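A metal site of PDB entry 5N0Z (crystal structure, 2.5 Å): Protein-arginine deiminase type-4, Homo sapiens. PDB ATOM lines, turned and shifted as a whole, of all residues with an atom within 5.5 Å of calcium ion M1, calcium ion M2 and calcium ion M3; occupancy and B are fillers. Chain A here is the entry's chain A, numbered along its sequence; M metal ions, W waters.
The side-chain amino group (NZ) of Lys 369 is in salt-bridge range of the side-chain carboxylate (OD2) of Asp 395 (3.2 Å). The backbone carbonyl oxygen (O) of Asn 160 lies within hydrogen-bond range of the side-chain sulfur (SG) of Cys 173. The side-chain amide nitrogen of Asn 160 sits at hydrogen-bond distance from the side-chain carboxylate of Glu 259, at 2.7 Å.
Six residues have an atom within 4 Å of calcium ion M1: Asn 160, Asp 162, Asp 164, Asp 172, Asp 183 and Asp 186. The nearest printed residue that does not touch calcium ion M1 is Arg 163 (5.4 Å).
Within 4 Å of calcium ion M2: Asp 162, Asp 164, Asp 186 and Asp 395.
Four residues have an atom within 4 Å of calcium ion M3: Asp 172, Asp 175, Glu 177 and Asp 183.
Calcium ion M1 is bound by the side-chain carboxylate (OD2) of Asp 172, at 2.1 Å. OD2 of Asp 186 is bound to calcium ion M1, at 2.3 Å. Calcium ion M1 is bound by OD1 of Asp 162, at 2.4 Å. OD1 of Asp 183 is bound to calcium ion M1 (2.5 Å). OD1 of Asn 160 binds calcium ion M1 (2.6 Å). OD2 of Asp 164 binds calcium ion M1. Calcium ion M1 has six donor atoms within binding distance.
Calcium ion M2 is bound by the side-chain carboxylate (OD2) of Asp 162 (2.3 Å), the side-chain carboxylate (OD1) of Asp 395 (2.3 Å), the side-chain carboxylate (OD2) of Asp 186 (2.4 Å), water W1 (2.4 Å), the side-chain carboxylate (OD2) of Asp 164 (2.6 Å) and the side-chain carboxylate (OD1) of Asp 186 (2.7 Å). Calcium ion M2 has six donor atoms within binding distance. Slightly farther from calcium ion M2 lies OD1 of Asp 164 (3.0 Å).
Water W3 binds calcium ion M3 (2.0 Å). The backbone carbonyl oxygen (O) of Glu 177 binds calcium ion M3 (2.3 Å). The backbone carbonyl oxygen (O) of Asp 172 binds calcium ion M3, 2.3 Å away. Calcium ion M3 is bound by the side-chain carboxylate (OD1) of Asp 175 (2.4 Å). Water W4 is bound to calcium ion M3, 2.5 Å away. Water W2 is bound to calcium ion M3, 2.5 Å away.
Water W4 bridges O of Asp 175 (2.7 Å) and OE2 of Glu 259 (3.1 Å). Water W3 bridges OD2 of Asp 183 and OE1 of Glu 259.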
ATOM      1  N   ASN A 160      27.056  26.150  -2.094  1.00  0.00           N
ATOM      2  CA  ASN A 160      25.978  26.948  -2.650  1.00  0.00           C
ATOM      3  C   ASN A 160      25.900  28.294  -1.927  1.00  0.00           C
ATOM      4  O   ASN A 160      24.955  28.603  -1.238  1.00  0.00           O
ATOM      5  CB  ASN A 160      24.670  26.147  -2.565  1.00  0.00           C
ATOM      6  CG  ASN A 160      23.565  26.742  -3.386  1.00  0.00           C
ATOM      7  OD1 ASN A 160      23.813  27.308  -4.444  1.00  0.00           O
ATOM      8  ND2 ASN A 160      22.335  26.594  -2.909  1.00  0.00           N
ATOM      9  N   ASP A 162      26.244  31.475  -3.277  1.00  0.00           N
ATOM     10  CA  ASP A 162      25.676  32.642  -3.986  1.00  0.00           C
ATOM     11  C   ASP A 162      24.249  32.964  -3.508  1.00  0.00           C
ATOM     12  O   ASP A 162      23.670  32.259  -2.672  1.00  0.00           O
ATOM     13  CB  ASP A 162      25.778  32.496  -5.538  1.00  0.00           C
ATOM     14  CG  ASP A 162      24.839  31.435  -6.114  1.00  0.00           C
ATOM     15  OD1 ASP A 162      24.111  30.787  -5.323  1.00  0.00           O
ATOM     16  OD2 ASP A 162      24.838  31.204  -7.360  1.00  0.00           O
ATOM     17  N   ARG A 163      23.711  34.047  -4.064  1.00  0.00           N
ATOM     18  CA  ARG A 163      22.333  34.513  -3.814  1.00  0.00           C
ATOM     19  C   ARG A 163      21.631  34.572  -5.156  1.00  0.00           C
ATOM     20  O   ARG A 163      21.732  35.565  -5.891  1.00  0.00           O
ATOM     21  CB  ARG A 163      22.408  35.884  -3.161  1.00  0.00           C
ATOM     22  CG  ARG A 163      21.157  36.389  -2.485  1.00  0.00           C
ATOM     23  CD  ARG A 163      21.563  37.493  -1.523  1.00  0.00           C
ATOM     24  NE  ARG A 163      22.130  38.672  -2.179  1.00  0.00           N
ATOM     25  CZ  ARG A 163      22.819  39.662  -1.578  1.00  0.00           C
ATOM     26  NH1 ARG A 163      23.055  39.663  -0.257  1.00  0.00           N
ATOM     27  NH2 ARG A 163      23.293  40.658  -2.304  1.00  0.00           N
ATOM     28  N   ASP A 164      20.989  33.457  -5.519  1.00  0.00           N
ATOM     29  CA  ASP A 164      20.090  33.378  -6.681  1.00  0.00           C
ATOM     30  C   ASP A 164      18.727  33.934  -6.289  1.00  0.00           C
ATOM     31  O   ASP A 164      18.030  34.566  -7.101  1.00  0.00           O
ATOM     32  CB  ASP A 164      19.933  31.937  -7.182  1.00  0.00           C
ATOM     33  CG  ASP A 164      21.076  31.494  -8.047  1.00  0.00           C
ATOM     34  OD1 ASP A 164      21.622  32.298  -8.808  1.00  0.00           O
ATOM     35  OD2 ASP A 164      21.426  30.302  -8.006  1.00  0.00           O
ATOM     36  N   ASP A 172      22.074  31.138  -0.435  1.00  0.00           N
ATOM     37  CA  ASP A 172      21.071  30.108  -0.709  1.00  0.00           C
ATOM     38  C   ASP A 172      21.040  28.954   0.292  1.00  0.00           C
ATOM     39  O   ASP A 172      19.954  28.509   0.676  1.00  0.00           O
ATOM     40  CB  ASP A 172      21.312  29.510  -2.102  1.00  0.00           C
ATOM     41  CG  ASP A 172      21.084  30.491  -3.207  1.00  0.00           C
ATOM     42  OD1 ASP A 172      20.518  31.583  -2.954  1.00  0.00           O
ATOM     43  OD2 ASP A 172      21.474  30.186  -4.347  1.00  0.00           O
ATOM     44  N   CYS A 173      22.220  28.487   0.686  1.00  0.00           N
ATOM     45  CA  CYS A 173      22.405  27.266   1.473  1.00  0.00           C
ATOM     46  C   CYS A 173      22.203  27.416   2.996  1.00  0.00           C
ATOM     47  O   CYS A 173      22.257  26.415   3.729  1.00  0.00           O
ATOM     48  CB  CYS A 173      23.783  26.659   1.157  1.00  0.00           C
ATOM     49  SG  CYS A 173      25.252  27.628   1.651  1.00  0.00           S
ATOM     50  N   GLU A 174      21.967  28.646   3.485  1.00  0.00           N
ATOM     51  CA  GLU A 174      21.753  28.842   4.938  1.00  0.00           C
ATOM     52  C   GLU A 174      20.398  28.347   5.460  1.00  0.00           C
ATOM     53  O   GLU A 174      20.274  28.081   6.648  1.00  0.00           O
ATOM     54  CB  GLU A 174      22.035  30.297   5.358  1.00  0.00           C
ATOM     55  CG  GLU A 174      23.474  30.540   5.787  1.00  0.00           C
ATOM     56  CD  GLU A 174      24.002  31.944   5.491  1.00  0.00           C
ATOM     57  OE1 GLU A 174      23.202  32.910   5.383  1.00  0.00           O
ATOM     58  OE2 GLU A 174      25.244  32.106   5.407  1.00  0.00           O
ATOM     59  N   ASP A 175      19.393  28.188   4.597  1.00  0.00           N
ATOM     60  CA  ASP A 175      18.061  27.747   5.024  1.00  0.00           C
ATOM     61  C   ASP A 175      17.849  26.308   4.554  1.00  0.00           C
ATOM     62  O   ASP A 175      18.765  25.713   3.987  1.00  0.00           O
ATOM     63  CB  ASP A 175      16.986  28.669   4.420  1.00  0.00           C
ATOM     64  CG  ASP A 175      16.893  28.565   2.876  1.00  0.00           C
ATOM     65  OD1 ASP A 175      17.569  27.713   2.250  1.00  0.00           O
ATOM     66  OD2 ASP A 175      16.148  29.363   2.263  1.00  0.00           O
ATOM     67  N   ASP A 176      16.641  25.775   4.752  1.00  0.00           N
ATOM     68  CA  ASP A 176      16.322  24.379   4.375  1.00  0.00           C
ATOM     69  C   ASP A 176      15.537  24.157   3.057  1.00  0.00           C
ATOM     70  O   ASP A 176      15.078  23.028   2.815  1.00  0.00           O
ATOM     71  CB  ASP A 176      15.559  23.712   5.539  1.00  0.00           C
ATOM     72  CG  ASP A 176      16.452  23.373   6.722  1.00  0.00           C
ATOM     73  OD1 ASP A 176      17.630  22.979   6.539  1.00  0.00           O
ATOM     74  OD2 ASP A 176      15.951  23.472   7.867  1.00  0.00           O
ATOM     75  N   GLU A 177      15.407  25.182   2.197  1.00  0.00           N
ATOM     76  CA  GLU A 177      14.518  25.130   0.996  1.00  0.00           C
ATOM     77  C   GLU A 177      15.189  25.527  -0.329  1.00  0.00           C
ATOM     78  O   GLU A 177      16.080  26.388  -0.346  1.00  0.00           O
ATOM     79  CB  GLU A 177      13.306  26.062   1.170  1.00  0.00           C
ATOM     80  CG  GLU A 177      12.816  26.263   2.600  1.00  0.00           C
ATOM     81  CD  GLU A 177      11.501  27.032   2.670  1.00  0.00           C
ATOM     82  OE1 GLU A 177      10.515  26.605   2.018  1.00  0.00           O
ATOM     83  OE2 GLU A 177      11.450  28.037   3.394  1.00  0.00           O
ATOM     84  N   VAL A 178      14.737  24.917  -1.432  1.00  0.00           N
ATOM     85  CA  VAL A 178      14.988  25.400  -2.808  1.00  0.00           C
ATOM     86  C   VAL A 178      13.856  26.359  -3.194  1.00  0.00           C
ATOM     87  O   VAL A 178      12.710  25.934  -3.404  1.00  0.00           O
ATOM     88  CB  VAL A 178      15.003  24.264  -3.843  1.00  0.00           C
ATOM     89  CG1 VAL A 178      15.125  24.810  -5.254  1.00  0.00           C
ATOM     90  CG2 VAL A 178      16.125  23.290  -3.580  1.00  0.00           C
ATOM     91  N   LEU A 179      14.176  27.643  -3.330  1.00  0.00           N
ATOM     92  CA  LEU A 179      13.160  28.660  -3.596  1.00  0.00           C
ATOM     93  C   LEU A 179      13.058  28.997  -5.076  1.00  0.00           C
ATOM     94  O   LEU A 179      11.967  29.178  -5.582  1.00  0.00           O
ATOM     95  CB  LEU A 179      13.431  29.903  -2.758  1.00  0.00           C
ATOM     96  CG  LEU A 179      13.357  29.630  -1.260  1.00  0.00           C
ATOM     97  CD1 LEU A 179      13.888  30.818  -0.474  1.00  0.00           C
ATOM     98  CD2 LEU A 179      11.944  29.259  -0.799  1.00  0.00           C
ATOM     99  N   GLU A 182      16.395  28.054 -10.612  1.00  0.00           N
ATOM    100  CA  GLU A 182      17.748  28.442 -10.999  1.00  0.00           C
ATOM    101  C   GLU A 182      18.763  27.842 -10.037  1.00  0.00           C
ATOM    102  O   GLU A 182      19.832  27.367 -10.449  1.00  0.00           O
ATOM    103  CB  GLU A 182      17.936  29.979 -10.987  1.00  0.00           C
ATOM    104  CG  GLU A 182      17.390  30.751 -12.197  1.00  0.00           C
ATOM    105  CD  GLU A 182      15.878  30.996 -12.158  1.00  0.00           C
ATOM    106  OE1 GLU A 182      15.299  31.031 -13.257  1.00  0.00           O
ATOM    107  OE2 GLU A 182      15.278  31.135 -11.054  1.00  0.00           O
ATOM    108  N   ASP A 183      18.403  27.894  -8.748  1.00  0.00           N
ATOM    109  CA  ASP A 183      19.212  27.361  -7.649  1.00  0.00           C
ATOM    110  C   ASP A 183      19.683  25.925  -7.912  1.00  0.00           C
ATOM    111  O   ASP A 183      20.857  25.596  -7.665  1.00  0.00           O
ATOM    112  CB  ASP A 183      18.425  27.458  -6.315  1.00  0.00           C
ATOM    113  CG  ASP A 183      19.313  27.370  -5.080  1.00  0.00           C
ATOM    114  OD1 ASP A 183      20.510  27.684  -5.193  1.00  0.00           O
ATOM    115  OD2 ASP A 183      18.784  27.025  -3.981  1.00  0.00           O
ATOM    116  N   ASP A 186      23.086  25.064  -9.527  1.00  0.00           N
ATOM    117  CA  ASP A 186      24.272  25.049  -8.682  1.00  0.00           C
ATOM    118  C   ASP A 186      24.506  23.697  -8.006  1.00  0.00           C
ATOM    119  O   ASP A 186      25.643  23.349  -7.671  1.00  0.00           O
ATOM    120  CB  ASP A 186      24.183  26.183  -7.639  1.00  0.00           C
ATOM    121  CG  ASP A 186      24.172  27.567  -8.286  1.00  0.00           C
ATOM    122  OD1 ASP A 186      24.728  27.747  -9.415  1.00  0.00           O
ATOM    123  OD2 ASP A 186      23.566  28.496  -7.670  1.00  0.00           O
ATOM    124  N   PHE A 221      18.207  17.351  -1.294  1.00  0.00           N
ATOM    125  CA  PHE A 221      16.783  17.505  -1.595  1.00  0.00           C
ATOM    126  C   PHE A 221      16.273  16.393  -2.480  1.00  0.00           C
ATOM    127  O   PHE A 221      16.936  15.991  -3.447  1.00  0.00           O
ATOM    128  CB  PHE A 221      16.567  18.808  -2.322  1.00  0.00           C
ATOM    129  CG  PHE A 221      16.950  20.010  -1.534  1.00  0.00           C
ATOM    130  CD1 PHE A 221      16.075  20.555  -0.617  1.00  0.00           C
ATOM    131  CD2 PHE A 221      18.189  20.620  -1.737  1.00  0.00           C
ATOM    132  CE1 PHE A 221      16.423  21.679   0.106  1.00  0.00           C
ATOM    133  CE2 PHE A 221      18.542  21.757  -1.020  1.00  0.00           C
ATOM    134  CZ  PHE A 221      17.663  22.289  -0.098  1.00  0.00           C
ATOM    135  N   GLU A 259      23.743  20.139  -2.271  1.00  0.00           N
ATOM    136  CA  GLU A 259      24.540  21.335  -2.117  1.00  0.00           C
ATOM    137  C   GLU A 259      25.434  21.110  -0.919  1.00  0.00           C
ATOM    138  O   GLU A 259      25.040  20.471   0.036  1.00  0.00           O
ATOM    139  CB  GLU A 259      23.662  22.601  -1.892  1.00  0.00           C
ATOM    140  CG  GLU A 259      22.533  22.404  -0.869  1.00  0.00           C
ATOM    141  CD  GLU A 259      21.758  23.666  -0.458  1.00  0.00           C
ATOM    142  OE1 GLU A 259      21.534  24.578  -1.298  1.00  0.00           O
ATOM    143  OE2 GLU A 259      21.356  23.723   0.742  1.00  0.00           O
ATOM    144  N   LYS A 369      28.749  23.459 -13.462  1.00  0.00           N
ATOM    145  CA  LYS A 369      28.572  24.838 -13.029  1.00  0.00           C
ATOM    146  C   LYS A 369      29.891  25.442 -12.579  1.00  0.00           C
ATOM    147  O   LYS A 369      30.704  24.791 -11.971  1.00  0.00           O
ATOM    148  CB  LYS A 369      27.544  24.943 -11.906  1.00  0.00           C
ATOM    149  CG  LYS A 369      27.344  26.349 -11.352  1.00  0.00           C
ATOM    150  CD  LYS A 369      26.910  27.379 -12.393  1.00  0.00           C
ATOM    151  CE  LYS A 369      25.466  27.245 -12.822  1.00  0.00           C
ATOM    152  NZ  LYS A 369      24.995  28.527 -13.394  1.00  0.00           N
ATOM    153  N   LEU A 371      31.231  29.337 -11.103  1.00  0.00           N
ATOM    154  CA  LEU A 371      30.770  30.629 -10.770  1.00  0.00           C
ATOM    155  C   LEU A 371      31.750  31.359  -9.878  1.00  0.00           C
ATOM    156  O   LEU A 371      32.393  30.757  -9.025  1.00  0.00           O
ATOM    157  CB  LEU A 371      29.391  30.522 -10.153  1.00  0.00           C
ATOM    158  CG  LEU A 371      29.257  29.773  -8.842  1.00  0.00           C
ATOM    159  CD1 LEU A 371      29.313  30.777  -7.704  1.00  0.00           C
ATOM    160  CD2 LEU A 371      27.966  29.020  -8.681  1.00  0.00           C
ATOM    161  N   PRO A 394      23.268  36.826  -7.975  1.00  0.00           N
ATOM    162  CA  PRO A 394      22.937  35.768  -8.920  1.00  0.00           C
ATOM    163  C   PRO A 394      24.176  35.254  -9.640  1.00  0.00           C
ATOM    164  O   PRO A 394      24.776  36.001 -10.407  1.00  0.00           O
ATOM    165  CB  PRO A 394      21.979  36.463  -9.900  1.00  0.00           C
ATOM    166  CG  PRO A 394      21.316  37.516  -9.074  1.00  0.00           C
ATOM    167  CD  PRO A 394      22.314  37.959  -8.043  1.00  0.00           C
ATOM    168  N   ASP A 395      24.558  34.014  -9.386  1.00  0.00           N
ATOM    169  CA  ASP A 395      25.807  33.437  -9.924  1.00  0.00           C
ATOM    170  C   ASP A 395      27.084  34.194  -9.446  1.00  0.00           C
ATOM    171  O   ASP A 395      28.078  34.318 -10.179  1.00  0.00           O
ATOM    172  CB  ASP A 395      25.740  33.298 -11.468  1.00  0.00           C
ATOM    173  CG  ASP A 395      24.911  32.116 -11.923  1.00  0.00           C
ATOM    174  OD1 ASP A 395      24.164  31.542 -11.114  1.00  0.00           O
ATOM    175  OD2 ASP A 395      25.038  31.732 -13.097  1.00  0.00           O
HETATM  176 CA    CA M   1      22.498  29.069  -5.744  1.00  0.00          CA
HETATM  177 CA    CA M   2      23.757  30.290  -9.191  1.00  0.00          CA
HETATM  178 CA    CA M   3      18.094  27.393  -0.103  1.00  0.00          CA
HETATM  179  O   HOH W   1      22.094  29.261 -10.523  1.00  0.00           O
HETATM  180  O   HOH W   2      17.319  29.758  -0.265  1.00  0.00           O
HETATM  181  O   HOH W   3      19.107  26.329  -1.519  1.00  0.00           O
HETATM  182  O   HOH W   4      18.859  25.497   1.292  1.00  0.00           O
